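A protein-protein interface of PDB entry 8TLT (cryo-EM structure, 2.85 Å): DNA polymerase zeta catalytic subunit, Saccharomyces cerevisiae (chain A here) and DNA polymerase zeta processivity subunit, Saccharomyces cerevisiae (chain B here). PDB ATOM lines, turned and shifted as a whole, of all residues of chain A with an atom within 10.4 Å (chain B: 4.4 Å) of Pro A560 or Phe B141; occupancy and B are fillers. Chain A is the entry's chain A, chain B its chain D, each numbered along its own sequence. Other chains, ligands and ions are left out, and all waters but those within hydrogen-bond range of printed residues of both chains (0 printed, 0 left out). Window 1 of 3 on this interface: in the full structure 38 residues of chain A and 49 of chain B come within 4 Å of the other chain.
The side-chain hydroxyl (OH) of Tyr B57 lies within hydrogen-bond range of the backbone carbonyl oxygen (O) of Gly A558, at 2.8 Å. The backbone carbonyl oxygen of Phe A562 lies within hydrogen-bond range of the side-chain hydroxyl of Tyr B27 (3.2 Å).
The backbone NH (N) of Cys B78 sits at hydrogen-bond distance from the backbone carbonyl oxygen (O) of Glu B142 (2.9 Å).
Pro A560 touches just these residues of chain B: Tyr B27 (3.2 Å) and Phe B141 (3.7 Å). Phe B141 touches just one residue of chain A: Pro A560 (3.7 Å). No residue of chain A comes within 4 Å of Thr B140. Of chain A, only Val A556 (3.5 Å) comes within 4 Å of Glu B142. Of the printed residues of chain A, Tyr B57 touches Tyr A557 and Gly A558. Of the printed residues of chain A, Val B26 touches Tyr A564. Of the printed residues of chain B, Gly A563 touches Tyr B27 (3.4 Å). Printed residues of chain B within 4 Å of Gly A558: Tyr B57. Ile B79 touches none of the printed residues of chain A.
CE1 of Tyr A550 touches SG of Cys B78, 3.7 Å away. CG1 of Val A556 touches CG of Glu B142, at 3.5 Å. Tyr B57 touches Tyr A557. Pro A560 touches Tyr B27. CB of Pro A560 touches CE1 of Phe B141, at 3.7 Å. Tyr B27 touches Gly A563 (CE1 to O, 3.4 Å). CD2 of Tyr A564 touches O of Val B26, at 3.5 Å. C of Tyr B27 touches CE2 of Tyr A564, 3.7 Å away. Tyr B27 touches Ile A567.
Of the 12 printed residues of chain A, 9 touch a printed residue of chain B. Along chain A the printed residues that touch a printed residue of chain B span positions 550 to 567. Hydrophobic or aromatic side chains of chain B within 4 Å of the printed part of chain A: Tyr B27, Tyr B57 and Phe B141. Among the printed residues, 11 pairs touch across the chains. Among the printed residues, no Asp or Glu carboxylate lies within 4 Å of a Lys or Arg side-chain nitrogen of the other chain.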
ATOM      1  N   TYR A 550       2.152  16.905  18.694  1.00  0.00           N
ATOM      2  CA  TYR A 550       2.723  17.077  20.026  1.00  0.00           C
ATOM      3  C   TYR A 550       2.495  18.488  20.556  1.00  0.00           C
ATOM      4  O   TYR A 550       2.203  18.669  21.744  1.00  0.00           O
ATOM      5  CB  TYR A 550       4.213  16.742  20.002  1.00  0.00           C
ATOM      6  CG  TYR A 550       4.496  15.261  19.887  1.00  0.00           C
ATOM      7  CD1 TYR A 550       3.702  14.332  20.544  1.00  0.00           C
ATOM      8  CD2 TYR A 550       5.558  14.793  19.126  1.00  0.00           C
ATOM      9  CE1 TYR A 550       3.952  12.978  20.445  1.00  0.00           C
ATOM     10  CE2 TYR A 550       5.817  13.439  19.021  1.00  0.00           C
ATOM     11  CZ  TYR A 550       5.012  12.538  19.683  1.00  0.00           C
ATOM     12  N   VAL A 556      10.846  15.998  23.842  1.00  0.00           N
ATOM     13  CA  VAL A 556      10.686  14.552  23.925  1.00  0.00           C
ATOM     14  C   VAL A 556      11.713  14.004  24.905  1.00  0.00           C
ATOM     15  O   VAL A 556      12.903  14.331  24.816  1.00  0.00           O
ATOM     16  CB  VAL A 556      10.838  13.891  22.544  1.00  0.00           C
ATOM     17  CG1 VAL A 556      10.165  12.537  22.530  1.00  0.00           C
ATOM     18  CG2 VAL A 556      10.259  14.789  21.462  1.00  0.00           C
ATOM     19  N   TYR A 557      11.255  13.175  25.839  1.00  0.00           N
ATOM     20  CA  TYR A 557      12.135  12.562  26.819  1.00  0.00           C
ATOM     21  C   TYR A 557      12.812  11.325  26.234  1.00  0.00           C
ATOM     22  O   TYR A 557      12.430  10.808  25.180  1.00  0.00           O
ATOM     23  CB  TYR A 557      11.358  12.193  28.082  1.00  0.00           C
ATOM     24  CG  TYR A 557      12.205  12.136  29.332  1.00  0.00           C
ATOM     25  CD1 TYR A 557      12.975  13.221  29.722  1.00  0.00           C
ATOM     26  CD2 TYR A 557      12.231  10.998  30.125  1.00  0.00           C
ATOM     27  CE1 TYR A 557      13.747  13.175  30.864  1.00  0.00           C
ATOM     28  CE2 TYR A 557      13.001  10.943  31.268  1.00  0.00           C
ATOM     29  CZ  TYR A 557      13.757  12.034  31.632  1.00  0.00           C
ATOM     30  OH  TYR A 557      14.526  11.984  32.771  1.00  0.00           O
ATOM     31  N   GLY A 558      13.833  10.844  26.941  1.00  0.00           N
ATOM     32  CA  GLY A 558      14.548   9.669  26.495  1.00  0.00           C
ATOM     33  C   GLY A 558      13.689   8.420  26.526  1.00  0.00           C
ATOM     34  O   GLY A 558      12.717   8.310  27.273  1.00  0.00           O
ATOM     35  N   GLU A 559      14.063   7.461  25.684  1.00  0.00           N
ATOM     36  CA  GLU A 559      13.307   6.226  25.580  1.00  0.00           C
ATOM     37  C   GLU A 559      13.403   5.427  26.880  1.00  0.00           C
ATOM     38  O   GLU A 559      14.431   5.456  27.561  1.00  0.00           O
ATOM     39  CB  GLU A 559      13.818   5.384  24.413  1.00  0.00           C
ATOM     40  N   PRO A 560      12.338   4.719  27.251  1.00  0.00           N
ATOM     41  CA  PRO A 560      12.390   3.913  28.465  1.00  0.00           C
ATOM     42  C   PRO A 560      13.408   2.801  28.323  1.00  0.00           C
ATOM     43  O   PRO A 560      13.655   2.298  27.210  1.00  0.00           O
ATOM     44  CB  PRO A 560      10.962   3.363  28.585  1.00  0.00           C
ATOM     45  CG  PRO A 560      10.404   3.440  27.210  1.00  0.00           C
ATOM     46  CD  PRO A 560      11.022   4.654  26.596  1.00  0.00           C
ATOM     47  N   PRO A 561      14.037   2.390  29.427  1.00  0.00           N
ATOM     48  CA  PRO A 561      15.082   1.358  29.331  1.00  0.00           C
ATOM     49  C   PRO A 561      14.589   0.026  28.796  1.00  0.00           C
ATOM     50  O   PRO A 561      15.346  -0.675  28.114  1.00  0.00           O
ATOM     51  CB  PRO A 561      15.578   1.232  30.780  1.00  0.00           C
ATOM     52  CG  PRO A 561      14.430   1.701  31.612  1.00  0.00           C
ATOM     53  CD  PRO A 561      13.777   2.791  30.819  1.00  0.00           C
ATOM     54  N   PHE A 562      13.347  -0.347  29.082  1.00  0.00           N
ATOM     55  CA  PHE A 562      12.823  -1.666  28.762  1.00  0.00           C
ATOM     56  C   PHE A 562      11.771  -1.579  27.665  1.00  0.00           C
ATOM     57  O   PHE A 562      11.323  -0.500  27.273  1.00  0.00           O
ATOM     58  CB  PHE A 562      12.222  -2.331  30.008  1.00  0.00           C
ATOM     59  CG  PHE A 562      13.119  -2.306  31.213  1.00  0.00           C
ATOM     60  CD1 PHE A 562      12.584  -2.372  32.484  1.00  0.00           C
ATOM     61  CD2 PHE A 562      14.498  -2.281  31.076  1.00  0.00           C
ATOM     62  CE1 PHE A 562      13.399  -2.358  33.593  1.00  0.00           C
ATOM     63  CE2 PHE A 562      15.317  -2.274  32.183  1.00  0.00           C
ATOM     64  CZ  PHE A 562      14.766  -2.315  33.443  1.00  0.00           C
ATOM     65  N   GLY A 563      11.385  -2.751  27.170  1.00  0.00           N
ATOM     66  CA  GLY A 563      10.284  -2.871  26.238  1.00  0.00           C
ATOM     67  C   GLY A 563       9.207  -3.772  26.803  1.00  0.00           C
ATOM     68  O   GLY A 563       9.279  -4.163  27.971  1.00  0.00           O
ATOM     69  N   TYR A 564       8.205  -4.112  25.992  1.00  0.00           N
ATOM     70  CA  TYR A 564       7.135  -4.971  26.486  1.00  0.00           C
ATOM     71  C   TYR A 564       7.630  -6.382  26.777  1.00  0.00           C
ATOM     72  O   TYR A 564       7.154  -7.020  27.722  1.00  0.00           O
ATOM     73  CB  TYR A 564       5.983  -5.014  25.484  1.00  0.00           C
ATOM     74  CG  TYR A 564       4.746  -5.702  26.011  1.00  0.00           C
ATOM     75  CD1 TYR A 564       4.575  -7.072  25.870  1.00  0.00           C
ATOM     76  CD2 TYR A 564       3.749  -4.983  26.650  1.00  0.00           C
ATOM     77  CE1 TYR A 564       3.448  -7.704  26.351  1.00  0.00           C
ATOM     78  CE2 TYR A 564       2.619  -5.605  27.134  1.00  0.00           C
ATOM     79  CZ  TYR A 564       2.472  -6.965  26.981  1.00  0.00           C
ATOM     80  OH  TYR A 564       1.347  -7.590  27.463  1.00  0.00           O
ATOM     81  N   ASP A 566      11.085  -7.326  27.108  1.00  0.00           N
ATOM     82  CA  ASP A 566      12.318  -7.387  27.881  1.00  0.00           C
ATOM     83  C   ASP A 566      12.119  -7.093  29.361  1.00  0.00           C
ATOM     84  O   ASP A 566      13.032  -7.355  30.151  1.00  0.00           O
ATOM     85  CB  ASP A 566      13.346  -6.412  27.303  1.00  0.00           C
ATOM     86  N   ILE A 567      10.959  -6.568  29.760  1.00  0.00           N
ATOM     87  CA  ILE A 567      10.772  -6.152  31.147  1.00  0.00           C
ATOM     88  C   ILE A 567      10.743  -7.363  32.074  1.00  0.00           C
ATOM     89  O   ILE A 567      11.411  -7.381  33.113  1.00  0.00           O
ATOM     90  CB  ILE A 567       9.502  -5.293  31.289  1.00  0.00           C
ATOM     91  CG1 ILE A 567       9.162  -5.072  32.764  1.00  0.00           C
ATOM     92  CG2 ILE A 567       8.336  -5.926  30.554  1.00  0.00           C
ATOM     93  N   LEU B  21       0.463   3.421  32.549  1.00  0.00           N
ATOM     94  CA  LEU B  21       1.262   2.309  32.046  1.00  0.00           C
ATOM     95  C   LEU B  21       0.548   0.977  32.233  1.00  0.00           C
ATOM     96  O   LEU B  21       0.561   0.128  31.337  1.00  0.00           O
ATOM     97  CB  LEU B  21       2.622   2.289  32.743  1.00  0.00           C
ATOM     98  CG  LEU B  21       3.816   2.866  31.981  1.00  0.00           C
ATOM     99  CD1 LEU B  21       3.454   4.180  31.315  1.00  0.00           C
ATOM    100  CD2 LEU B  21       4.997   3.049  32.916  1.00  0.00           C
ATOM    101  N   VAL B  26       1.537  -0.874  27.533  1.00  0.00           N
ATOM    102  CA  VAL B  26       2.930  -0.524  27.281  1.00  0.00           C
ATOM    103  C   VAL B  26       3.849  -1.490  28.013  1.00  0.00           C
ATOM    104  O   VAL B  26       4.927  -1.833  27.514  1.00  0.00           O
ATOM    105  CB  VAL B  26       3.203   0.936  27.678  1.00  0.00           C
ATOM    106  CG1 VAL B  26       2.716   1.874  26.592  1.00  0.00           C
ATOM    107  CG2 VAL B  26       2.522   1.252  28.973  1.00  0.00           C
ATOM    108  N   TYR B  27       3.446  -1.941  29.199  1.00  0.00           N
ATOM    109  CA  TYR B  27       4.126  -2.999  29.923  1.00  0.00           C
ATOM    110  C   TYR B  27       3.093  -4.006  30.410  1.00  0.00           C
ATOM    111  O   TYR B  27       1.976  -3.621  30.775  1.00  0.00           O
ATOM    112  CB  TYR B  27       4.922  -2.434  31.105  1.00  0.00           C
ATOM    113  CG  TYR B  27       6.097  -1.592  30.672  1.00  0.00           C
ATOM    114  CD1 TYR B  27       7.189  -2.168  30.038  1.00  0.00           C
ATOM    115  CD2 TYR B  27       6.110  -0.223  30.883  1.00  0.00           C
ATOM    116  CE1 TYR B  27       8.261  -1.404  29.634  1.00  0.00           C
ATOM    117  CE2 TYR B  27       7.179   0.548  30.482  1.00  0.00           C
ATOM    118  CZ  TYR B  27       8.252  -0.047  29.859  1.00  0.00           C
ATOM    119  OH  TYR B  27       9.320   0.720  29.459  1.00  0.00           O
ATOM    120  N   TYR B  57      13.589   5.359  36.776  1.00  0.00           N
ATOM    121  CA  TYR B  57      13.462   6.192  35.585  1.00  0.00           C
ATOM    122  C   TYR B  57      12.247   7.108  35.680  1.00  0.00           C
ATOM    123  O   TYR B  57      12.329   8.301  35.361  1.00  0.00           O
ATOM    124  CB  TYR B  57      13.381   5.301  34.345  1.00  0.00           C
ATOM    125  CG  TYR B  57      12.831   5.973  33.108  1.00  0.00           C
ATOM    126  CD1 TYR B  57      13.581   6.910  32.413  1.00  0.00           C
ATOM    127  CD2 TYR B  57      11.570   5.654  32.624  1.00  0.00           C
ATOM    128  CE1 TYR B  57      13.085   7.520  31.278  1.00  0.00           C
ATOM    129  CE2 TYR B  57      11.067   6.259  31.490  1.00  0.00           C
ATOM    130  CZ  TYR B  57      11.828   7.191  30.822  1.00  0.00           C
ATOM    131  OH  TYR B  57      11.333   7.798  29.691  1.00  0.00           O
ATOM    132  N   ILE B  77       1.588  12.327  28.595  1.00  0.00           N
ATOM    133  CA  ILE B  77       2.103  10.987  28.347  1.00  0.00           C
ATOM    134  C   ILE B  77       1.477  10.517  27.045  1.00  0.00           C
ATOM    135  O   ILE B  77       0.260  10.307  26.969  1.00  0.00           O
ATOM    136  CB  ILE B  77       1.786  10.028  29.502  1.00  0.00           C
ATOM    137  CG1 ILE B  77       2.621  10.376  30.737  1.00  0.00           C
ATOM    138  CG2 ILE B  77       2.036   8.589  29.086  1.00  0.00           C
ATOM    139  CD1 ILE B  77       4.063  10.708  30.434  1.00  0.00           C
ATOM    140  N   CYS B  78       2.301  10.351  26.016  1.00  0.00           N
ATOM    141  CA  CYS B  78       1.828  10.053  24.673  1.00  0.00           C
ATOM    142  C   CYS B  78       1.919   8.559  24.405  1.00  0.00           C
ATOM    143  O   CYS B  78       2.970   7.947  24.619  1.00  0.00           O
ATOM    144  CB  CYS B  78       2.638  10.826  23.633  1.00  0.00           C
ATOM    145  SG  CYS B  78       2.554  12.619  23.813  1.00  0.00           S
ATOM    146  N   ILE B  79       0.819   7.979  23.941  1.00  0.00           N
ATOM    147  CA  ILE B  79       0.779   6.576  23.546  1.00  0.00           C
ATOM    148  C   ILE B  79       1.066   6.507  22.052  1.00  0.00           C
ATOM    149  O   ILE B  79       0.344   7.103  21.246  1.00  0.00           O
ATOM    150  CB  ILE B  79      -0.580   5.944  23.880  1.00  0.00           C
ATOM    151  CG1 ILE B  79      -0.665   5.609  25.369  1.00  0.00           C
ATOM    152  CG2 ILE B  79      -0.815   4.703  23.037  1.00  0.00           C
ATOM    153  CD1 ILE B  79       0.395   4.651  25.839  1.00  0.00           C
ATOM    154  N   THR B 140       3.636   1.815  22.936  1.00  0.00           N
ATOM    155  CA  THR B 140       4.826   2.435  23.498  1.00  0.00           C
ATOM    156  C   THR B 140       4.437   3.798  24.047  1.00  0.00           C
ATOM    157  O   THR B 140       3.510   4.439  23.546  1.00  0.00           O
ATOM    158  CB  THR B 140       5.946   2.575  22.460  1.00  0.00           C
ATOM    159  N   PHE B 141       5.146   4.236  25.082  1.00  0.00           N
ATOM    160  CA  PHE B 141       4.840   5.486  25.758  1.00  0.00           C
ATOM    161  C   PHE B 141       6.031   6.432  25.686  1.00  0.00           C
ATOM    162  O   PHE B 141       7.183   6.001  25.593  1.00  0.00           O
ATOM    163  CB  PHE B 141       4.439   5.248  27.222  1.00  0.00           C
ATOM    164  CG  PHE B 141       5.550   5.486  28.207  1.00  0.00           C
ATOM    165  CD1 PHE B 141       6.547   4.545  28.387  1.00  0.00           C
ATOM    166  CD2 PHE B 141       5.590   6.649  28.957  1.00  0.00           C
ATOM    167  CE1 PHE B 141       7.565   4.762  29.294  1.00  0.00           C
ATOM    168  CE2 PHE B 141       6.605   6.870  29.864  1.00  0.00           C
ATOM    169  CZ  PHE B 141       7.593   5.926  30.032  1.00  0.00           C
ATOM    170  N   GLU B 142       5.735   7.727  25.727  1.00  0.00           N
ATOM    171  CA  GLU B 142       6.756   8.762  25.683  1.00  0.00           C
ATOM    172  C   GLU B 142       6.298   9.963  26.496  1.00  0.00           C
ATOM    173  O   GLU B 142       5.139  10.375  26.408  1.00  0.00           O
ATOM    174  CB  GLU B 142       7.055   9.181  24.240  1.00  0.00           C
ATOM    175  CG  GLU B 142       7.762  10.511  24.108  1.00  0.00           C
